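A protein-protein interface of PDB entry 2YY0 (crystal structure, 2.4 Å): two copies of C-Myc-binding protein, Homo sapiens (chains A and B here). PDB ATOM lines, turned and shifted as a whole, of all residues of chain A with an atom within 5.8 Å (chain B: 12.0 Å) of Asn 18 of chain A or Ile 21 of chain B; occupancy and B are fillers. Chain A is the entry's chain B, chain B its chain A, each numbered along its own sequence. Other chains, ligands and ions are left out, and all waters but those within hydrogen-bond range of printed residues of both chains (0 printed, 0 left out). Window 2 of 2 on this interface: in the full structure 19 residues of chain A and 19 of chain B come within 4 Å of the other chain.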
ATOM      1  N   PRO A  16      -4.154 -31.866  33.522  1.00  0.00           N
ATOM      2  CA  PRO A  16      -5.005 -30.685  33.693  1.00  0.00           C
ATOM      3  C   PRO A  16      -4.515 -29.584  32.761  1.00  0.00           C
ATOM      4  O   PRO A  16      -3.308 -29.368  32.629  1.00  0.00           O
ATOM      5  CB  PRO A  16      -4.800 -30.318  35.160  1.00  0.00           C
ATOM      6  CG  PRO A  16      -4.476 -31.633  35.798  1.00  0.00           C
ATOM      7  CD  PRO A  16      -3.532 -32.249  34.800  1.00  0.00           C
ATOM      8  N   GLU A  17      -5.447 -28.896  32.112  1.00  0.00           N
ATOM      9  CA  GLU A  17      -5.085 -27.825  31.192  1.00  0.00           C
ATOM     10  C   GLU A  17      -4.402 -26.666  31.906  1.00  0.00           C
ATOM     11  O   GLU A  17      -5.048 -25.909  32.624  1.00  0.00           O
ATOM     12  CB  GLU A  17      -6.328 -27.313  30.454  1.00  0.00           C
ATOM     13  CG  GLU A  17      -6.483 -27.837  29.016  1.00  0.00           C
ATOM     14  CD  GLU A  17      -6.619 -29.350  28.930  1.00  0.00           C
ATOM     15  OE1 GLU A  17      -5.650 -30.060  29.291  1.00  0.00           O
ATOM     16  OE2 GLU A  17      -7.695 -29.825  28.499  1.00  0.00           O
ATOM     17  N   ASN A  18      -3.093 -26.538  31.717  1.00  0.00           N
ATOM     18  CA  ASN A  18      -2.349 -25.450  32.336  1.00  0.00           C
ATOM     19  C   ASN A  18      -2.368 -24.243  31.396  1.00  0.00           C
ATOM     20  O   ASN A  18      -1.932 -24.332  30.249  1.00  0.00           O
ATOM     21  CB  ASN A  18      -0.901 -25.864  32.606  1.00  0.00           C
ATOM     22  CG  ASN A  18      -0.110 -24.775  33.319  1.00  0.00           C
ATOM     23  OD1 ASN A  18      -0.141 -23.615  32.919  1.00  0.00           O
ATOM     24  ND2 ASN A  18       0.604 -25.148  34.376  1.00  0.00           N
ATOM     25  N   PRO A  19      -2.882 -23.101  31.873  1.00  0.00           N
ATOM     26  CA  PRO A  19      -2.981 -21.851  31.111  1.00  0.00           C
ATOM     27  C   PRO A  19      -1.640 -21.286  30.608  1.00  0.00           C
ATOM     28  O   PRO A  19      -1.584 -20.638  29.558  1.00  0.00           O
ATOM     29  CB  PRO A  19      -3.674 -20.910  32.091  1.00  0.00           C
ATOM     30  CG  PRO A  19      -4.506 -21.821  32.902  1.00  0.00           C
ATOM     31  CD  PRO A  19      -3.567 -22.971  33.165  1.00  0.00           C
ATOM     32  N   GLU A  20      -0.567 -21.523  31.358  1.00  0.00           N
ATOM     33  CA  GLU A  20       0.744 -21.037  30.960  1.00  0.00           C
ATOM     34  C   GLU A  20       1.211 -21.812  29.750  1.00  0.00           C
ATOM     35  O   GLU A  20       1.771 -21.237  28.821  1.00  0.00           O
ATOM     36  CB  GLU A  20       1.757 -21.184  32.103  1.00  0.00           C
ATOM     37  CG  GLU A  20       3.164 -20.721  31.751  1.00  0.00           C
ATOM     38  CD  GLU A  20       3.201 -19.315  31.143  1.00  0.00           C
ATOM     39  OE1 GLU A  20       4.302 -18.853  30.755  1.00  0.00           O
ATOM     40  OE2 GLU A  20       2.134 -18.666  31.046  1.00  0.00           O
ATOM     41  N   ILE A  21       0.964 -23.117  29.747  1.00  0.00           N
ATOM     42  CA  ILE A  21       1.374 -23.958  28.633  1.00  0.00           C
ATOM     43  C   ILE A  21       0.608 -23.592  27.357  1.00  0.00           C
ATOM     44  O   ILE A  21       1.186 -23.532  26.271  1.00  0.00           O
ATOM     45  CB  ILE A  21       1.168 -25.436  28.978  1.00  0.00           C
ATOM     46  CG1 ILE A  21       2.116 -25.815  30.114  1.00  0.00           C
ATOM     47  CG2 ILE A  21       1.405 -26.325  27.750  1.00  0.00           C
ATOM     48  CD1 ILE A  21       2.007 -27.252  30.540  1.00  0.00           C
ATOM     49  N   GLU A  22      -0.686 -23.321  27.486  1.00  0.00           N
ATOM     50  CA  GLU A  22      -1.496 -22.958  26.321  1.00  0.00           C
ATOM     51  C   GLU A  22      -0.993 -21.642  25.720  1.00  0.00           C
ATOM     52  O   GLU A  22      -0.920 -21.506  24.498  1.00  0.00           O
ATOM     53  CB  GLU A  22      -2.962 -22.847  26.732  1.00  0.00           C
ATOM     54  CG  GLU A  22      -3.472 -24.120  27.389  1.00  0.00           C
ATOM     55  CD  GLU A  22      -4.850 -23.966  27.992  1.00  0.00           C
ATOM     56  OE1 GLU A  22      -5.035 -23.018  28.787  1.00  0.00           O
ATOM     57  OE2 GLU A  22      -5.740 -24.796  27.679  1.00  0.00           O
ATOM     58  N   LEU A  23      -0.639 -20.687  26.581  1.00  0.00           N
ATOM     59  CA  LEU A  23      -0.111 -19.415  26.125  1.00  0.00           C
ATOM     60  C   LEU A  23       1.143 -19.653  25.305  1.00  0.00           C
ATOM     61  O   LEU A  23       1.195 -19.305  24.129  1.00  0.00           O
ATOM     62  CB  LEU A  23       0.254 -18.516  27.303  1.00  0.00           C
ATOM     63  CG  LEU A  23      -0.673 -17.376  27.729  1.00  0.00           C
ATOM     64  CD1 LEU A  23       0.074 -16.557  28.789  1.00  0.00           C
ATOM     65  CD2 LEU A  23      -1.068 -16.469  26.553  1.00  0.00           C
ATOM     66  N   LEU A  24       2.147 -20.254  25.941  1.00  0.00           N
ATOM     67  CA  LEU A  24       3.424 -20.553  25.306  1.00  0.00           C
ATOM     68  C   LEU A  24       3.253 -21.298  23.978  1.00  0.00           C
ATOM     69  O   LEU A  24       3.952 -21.015  22.982  1.00  0.00           O
ATOM     70  CB  LEU A  24       4.301 -21.372  26.266  1.00  0.00           C
ATOM     71  CG  LEU A  24       5.038 -20.617  27.372  1.00  0.00           C
ATOM     72  CD1 LEU A  24       5.571 -21.574  28.397  1.00  0.00           C
ATOM     73  CD2 LEU A  24       6.198 -19.821  26.748  1.00  0.00           C
ATOM     74  N   PRO B  16       7.354 -20.787  35.916  1.00  0.00           N
ATOM     75  CA  PRO B  16       7.305 -21.925  36.875  1.00  0.00           C
ATOM     76  C   PRO B  16       8.410 -22.936  36.587  1.00  0.00           C
ATOM     77  O   PRO B  16       8.667 -23.255  35.434  1.00  0.00           O
ATOM     78  CB  PRO B  16       5.932 -22.573  36.724  1.00  0.00           C
ATOM     79  CG  PRO B  16       5.091 -21.398  36.167  1.00  0.00           C
ATOM     80  CD  PRO B  16       6.050 -20.636  35.237  1.00  0.00           C
ATOM     81  N   GLU B  17       9.062 -23.437  37.634  1.00  0.00           N
ATOM     82  CA  GLU B  17      10.140 -24.426  37.479  1.00  0.00           C
ATOM     83  C   GLU B  17       9.589 -25.804  37.087  1.00  0.00           C
ATOM     84  O   GLU B  17       9.843 -26.819  37.751  1.00  0.00           O
ATOM     85  CB  GLU B  17      10.960 -24.552  38.771  1.00  0.00           C
ATOM     86  CG  GLU B  17      11.708 -23.284  39.183  1.00  0.00           C
ATOM     87  CD  GLU B  17      12.761 -22.860  38.173  1.00  0.00           C
ATOM     88  OE1 GLU B  17      13.511 -21.907  38.465  1.00  0.00           O
ATOM     89  OE2 GLU B  17      12.840 -23.471  37.088  1.00  0.00           O
ATOM     90  N   ASN B  18       8.829 -25.818  35.998  1.00  0.00           N
ATOM     91  CA  ASN B  18       8.232 -27.029  35.464  1.00  0.00           C
ATOM     92  C   ASN B  18       9.058 -27.371  34.240  1.00  0.00           C
ATOM     93  O   ASN B  18       9.343 -26.503  33.419  1.00  0.00           O
ATOM     94  CB  ASN B  18       6.772 -26.754  35.063  1.00  0.00           C
ATOM     95  CG  ASN B  18       6.111 -27.924  34.332  1.00  0.00           C
ATOM     96  OD1 ASN B  18       4.910 -27.894  34.085  1.00  0.00           O
ATOM     97  ND2 ASN B  18       6.885 -28.943  33.980  1.00  0.00           N
ATOM     98  N   PRO B  19       9.486 -28.632  34.121  1.00  0.00           N
ATOM     99  CA  PRO B  19      10.279 -29.006  32.957  1.00  0.00           C
ATOM    100  C   PRO B  19       9.547 -28.741  31.632  1.00  0.00           C
ATOM    101  O   PRO B  19      10.121 -28.159  30.713  1.00  0.00           O
ATOM    102  CB  PRO B  19      10.568 -30.479  33.216  1.00  0.00           C
ATOM    103  CG  PRO B  19      10.705 -30.508  34.721  1.00  0.00           C
ATOM    104  CD  PRO B  19       9.521 -29.694  35.143  1.00  0.00           C
ATOM    105  N   GLU B  20       8.277 -29.123  31.540  1.00  0.00           N
ATOM    106  CA  GLU B  20       7.516 -28.906  30.304  1.00  0.00           C
ATOM    107  C   GLU B  20       7.391 -27.430  29.914  1.00  0.00           C
ATOM    108  O   GLU B  20       7.519 -27.068  28.741  1.00  0.00           O
ATOM    109  CB  GLU B  20       6.121 -29.518  30.425  1.00  0.00           C
ATOM    110  CG  GLU B  20       5.332 -29.473  29.128  1.00  0.00           C
ATOM    111  CD  GLU B  20       6.133 -30.032  27.960  1.00  0.00           C
ATOM    112  OE1 GLU B  20       6.759 -31.106  28.135  1.00  0.00           O
ATOM    113  OE2 GLU B  20       6.137 -29.402  26.875  1.00  0.00           O
ATOM    114  N   ILE B  21       7.120 -26.588  30.902  1.00  0.00           N
ATOM    115  CA  ILE B  21       6.997 -25.155  30.693  1.00  0.00           C
ATOM    116  C   ILE B  21       8.344 -24.573  30.257  1.00  0.00           C
ATOM    117  O   ILE B  21       8.419 -23.850  29.254  1.00  0.00           O
ATOM    118  CB  ILE B  21       6.507 -24.484  31.997  1.00  0.00           C
ATOM    119  CG1 ILE B  21       5.007 -24.764  32.148  1.00  0.00           C
ATOM    120  CG2 ILE B  21       6.849 -22.982  32.020  1.00  0.00           C
ATOM    121  CD1 ILE B  21       4.410 -24.359  33.477  1.00  0.00           C
ATOM    122  N   GLU B  22       9.407 -24.901  30.998  1.00  0.00           N
ATOM    123  CA  GLU B  22      10.744 -24.428  30.676  1.00  0.00           C
ATOM    124  C   GLU B  22      11.174 -24.913  29.299  1.00  0.00           C
ATOM    125  O   GLU B  22      11.839 -24.181  28.573  1.00  0.00           O
ATOM    126  CB  GLU B  22      11.761 -24.896  31.726  1.00  0.00           C
ATOM    127  CG  GLU B  22      11.691 -24.166  33.066  1.00  0.00           C
ATOM    128  CD  GLU B  22      11.424 -22.662  32.929  1.00  0.00           C
ATOM    129  OE1 GLU B  22      11.949 -22.016  31.989  1.00  0.00           O
ATOM    130  OE2 GLU B  22      10.691 -22.121  33.779  1.00  0.00           O
ATOM    131  N   LEU B  23      10.814 -26.146  28.942  1.00  0.00           N
ATOM    132  CA  LEU B  23      11.150 -26.689  27.616  1.00  0.00           C
ATOM    133  C   LEU B  23      10.450 -25.803  26.567  1.00  0.00           C
ATOM    134  O   LEU B  23      11.058 -25.370  25.581  1.00  0.00           O
ATOM    135  CB  LEU B  23      10.659 -28.149  27.478  1.00  0.00           C
ATOM    136  CG  LEU B  23      10.955 -28.920  26.178  1.00  0.00           C
ATOM    137  CD1 LEU B  23      10.297 -30.274  26.218  1.00  0.00           C
ATOM    138  CD2 LEU B  23      10.410 -28.178  24.990  1.00  0.00           C
ATOM    139  N   LEU B  24       9.170 -25.536  26.773  1.00  0.00           N
ATOM    140  CA  LEU B  24       8.456 -24.668  25.838  1.00  0.00           C
ATOM    141  C   LEU B  24       9.119 -23.298  25.722  1.00  0.00           C
ATOM    142  O   LEU B  24       9.171 -22.730  24.634  1.00  0.00           O
ATOM    143  CB  LEU B  24       7.008 -24.477  26.279  1.00  0.00           C
ATOM    144  CG  LEU B  24       5.937 -25.212  25.480  1.00  0.00           C
ATOM    145  CD1 LEU B  24       6.383 -26.602  25.116  1.00  0.00           C
ATOM    146  CD2 LEU B  24       4.668 -25.255  26.311  1.00  0.00           C
ATOM    147  N   ARG B  25       9.614 -22.758  26.835  1.00  0.00           N
ATOM    148  CA  ARG B  25      10.247 -21.442  26.774  1.00  0.00           C
ATOM    149  C   ARG B  25      11.537 -21.518  25.989  1.00  0.00           C
ATOM    150  O   ARG B  25      11.927 -20.553  25.337  1.00  0.00           O
ATOM    151  CB  ARG B  25      10.555 -20.893  28.165  1.00  0.00           C
ATOM    152  CG  ARG B  25       9.357 -20.477  28.965  1.00  0.00           C
ATOM    153  CD  ARG B  25       9.827 -19.852  30.282  1.00  0.00           C
ATOM    154  NE  ARG B  25       8.747 -19.750  31.255  1.00  0.00           N
ATOM    155  CZ  ARG B  25       7.715 -18.923  31.143  1.00  0.00           C
ATOM    156  NH1 ARG B  25       7.622 -18.108  30.096  1.00  0.00           N
ATOM    157  NH2 ARG B  25       6.760 -18.931  32.065  1.00  0.00           N
ATOM    158  N   LEU B  26      12.193 -22.672  26.049  1.00  0.00           N
ATOM    159  CA  LEU B  26      13.450 -22.864  25.338  1.00  0.00           C
ATOM    160  C   LEU B  26      13.201 -22.906  23.833  1.00  0.00           C
ATOM    161  O   LEU B  26      13.952 -22.328  23.051  1.00  0.00           O
ATOM    162  CB  LEU B  26      14.151 -24.143  25.813  1.00  0.00           C
ATOM    163  CG  LEU B  26      15.405 -24.547  25.028  1.00  0.00           C
ATOM    164  CD1 LEU B  26      16.376 -23.361  24.959  1.00  0.00           C
ATOM    165  CD2 LEU B  26      16.065 -25.758  25.699  1.00  0.00           C
ATOM    166  N   GLU B  27      12.140 -23.578  23.430  1.00  0.00           N
ATOM    167  CA  GLU B  27      11.784 -23.648  22.017  1.00  0.00           C
ATOM    168  C   GLU B  27      11.351 -22.268  21.538  1.00  0.00           C
ATOM    169  O   GLU B  27      11.724 -21.845  20.453  1.00  0.00           O
ATOM    170  CB  GLU B  27      10.648 -24.642  21.793  1.00  0.00           C
ATOM    171  CG  GLU B  27      11.087 -26.093  21.735  1.00  0.00           C
ATOM    172  CD  GLU B  27       9.939 -27.046  22.019  1.00  0.00           C
ATOM    173  OE1 GLU B  27       8.830 -26.564  22.332  1.00  0.00           O
ATOM    174  OE2 GLU B  27      10.143 -28.274  21.945  1.00  0.00           O
ATOM    175  N   LEU B  28      10.584 -21.557  22.353  1.00  0.00           N
ATOM    176  CA  LEU B  28      10.143 -20.218  21.942  1.00  0.00           C
ATOM    177  C   LEU B  28      11.360 -19.307  21.723  1.00  0.00           C
ATOM    178  O   LEU B  28      11.435 -18.554  20.748  1.00  0.00           O
ATOM    179  CB  LEU B  28       9.212 -19.625  23.002  1.00  0.00           C
ATOM    180  CG  LEU B  28       8.596 -18.259  22.708  1.00  0.00           C
ATOM    181  CD1 LEU B  28       7.914 -18.288  21.339  1.00  0.00           C
ATOM    182  CD2 LEU B  28       7.627 -17.869  23.835  1.00  0.00           C
ATOM    183  N   ALA B  29      12.328 -19.417  22.620  1.00  0.00           N
ATOM    184  CA  ALA B  29      13.546 -18.621  22.546  1.00  0.00           C
ATOM    185  C   ALA B  29      14.394 -18.961  21.325  1.00  0.00           C
ATOM    186  O   ALA B  29      15.034 -18.083  20.745  1.00  0.00           O
ATOM    187  CB  ALA B  29      14.358 -18.819  23.829  1.00  0.00           C
ATOM    188  N   GLU B  30      14.412 -20.239  20.946  1.00  0.00           N
ATOM    189  CA  GLU B  30      15.172 -20.698  19.781  1.00  0.00           C
ATOM    190  C   GLU B  30      14.543 -20.187  18.491  1.00  0.00           C
ATOM    191  O   GLU B  30      15.238 -19.694  17.596  1.00  0.00           O
ATOM    192  CB  GLU B  30      15.215 -22.228  19.715  1.00  0.00           C
ATOM    193  CG  GLU B  30      16.301 -22.871  20.550  1.00  0.00           C
ATOM    194  CD  GLU B  30      16.500 -24.331  20.191  1.00  0.00           C
ATOM    195  OE1 GLU B  30      15.644 -25.164  20.568  1.00  0.00           O
ATOM    196  OE2 GLU B  30      17.506 -24.647  19.518  1.00  0.00           O
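The guanidinium group (NH2) of Arg 25 of chain B is in salt-bridge range of the side-chain carboxylate (OE1) of Glu 20 of chain A.
OD1 of Asn 18 of chain A lies within hydrogen-bond range of N of Ile 21 of chain A.
The side-chain carboxylate (OE2) of Glu 22 of chain B lies within salt-bridge range of the guanidinium group (NE) of Arg 25 of chain B.
OD1 of Asn 18 of chain A is in hydrogen-bond range of N of Glu 20 of chain A (2.6 Å).
Among the printed residues, merely in contact across the chains: Ile 21 of chain A with Ile 21 of chain B (3.7 Å), Ile 21 of chain A with Leu 24 of chain B (3.7 Å), Leu 24 of chain A with Ile 21 of chain B (3.7 Å), Leu 24 of chain A with Leu 28 of chain B (3.8 Å), Leu 24 of chain A with Leu 24 of chain B (3.9 Å), Leu 24 of chain A with Arg 25 of chain B (3.9 Å) and Asn 18 of chain A with Ile 21 of chain B (3.99 Å).
Of the printed residues of chain A, Ile 21 of chain B touches Asn 18 (3.99 Å), Ile 21 (3.7 Å) and Leu 24 (3.7 Å).
No residue of chain B comes within 4 Å of Glu 17 of chain A.
Of chain B, only Arg 25 (2.8 Å) comes within 4 Å of Glu 20 of chain A.
Ile 21 of chain A touches just these residues of chain B: Ile 21 (3.7 Å) and Leu 24 (3.7 Å).
No residue of chain B comes within 4 Å of Glu 22 of chain A.
Printed residues of chain A within 4 Å of Leu 24 of chain B: Ile 21 (3.7 Å) and Leu 24 (3.9 Å).
Of the printed residues of chain B, Leu 24 of chain A touches Ile 21, Leu 24, Arg 25 and Leu 28.
Leu 26 of chain B touches none of the printed residues of chain A.
The nearest printed residue of chain B that does not touch Asn 18 of chain A is Asn 18 of chain B (5.1 Å).
The nearest printed residue of chain B that does not touch Leu 24 of chain A is Glu 22 of chain B (5.7 Å).
Of the 9 printed residues of chain A, 4 touch a printed residue of chain B.
Hydrophobic or aromatic side chains of chain B within 4 Å of the printed part of chain A: Ile 21, Leu 24 and Leu 28.
Among the printed residues, Asp or Glu carboxylates within 4 Å of a Lys or Arg side-chain nitrogen of the other chain: Glu 20 of chain A with Arg 25 of chain B.
Asn 18 of chain A touches Ile 21 of chain B, but with the chains exchanged Ile 21 of chain A does not touch Asn 18 of chain B (4.6 Å).
Ile 21 of chain B touches its own counterpart, Ile 21 of chain A.
Ile 21 of chain A touches Leu 24 of chain B, and with the chains exchanged Leu 24 of chain A touches Ile 21 of chain B.
Leu 24 of chain A touches its own counterpart, Leu 24 of chain B.
9 positions are printed for both chains.
Of the 8 pairs that touch across the chains among the printed residues, 4 have their exchanged pair printed and touching as well.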
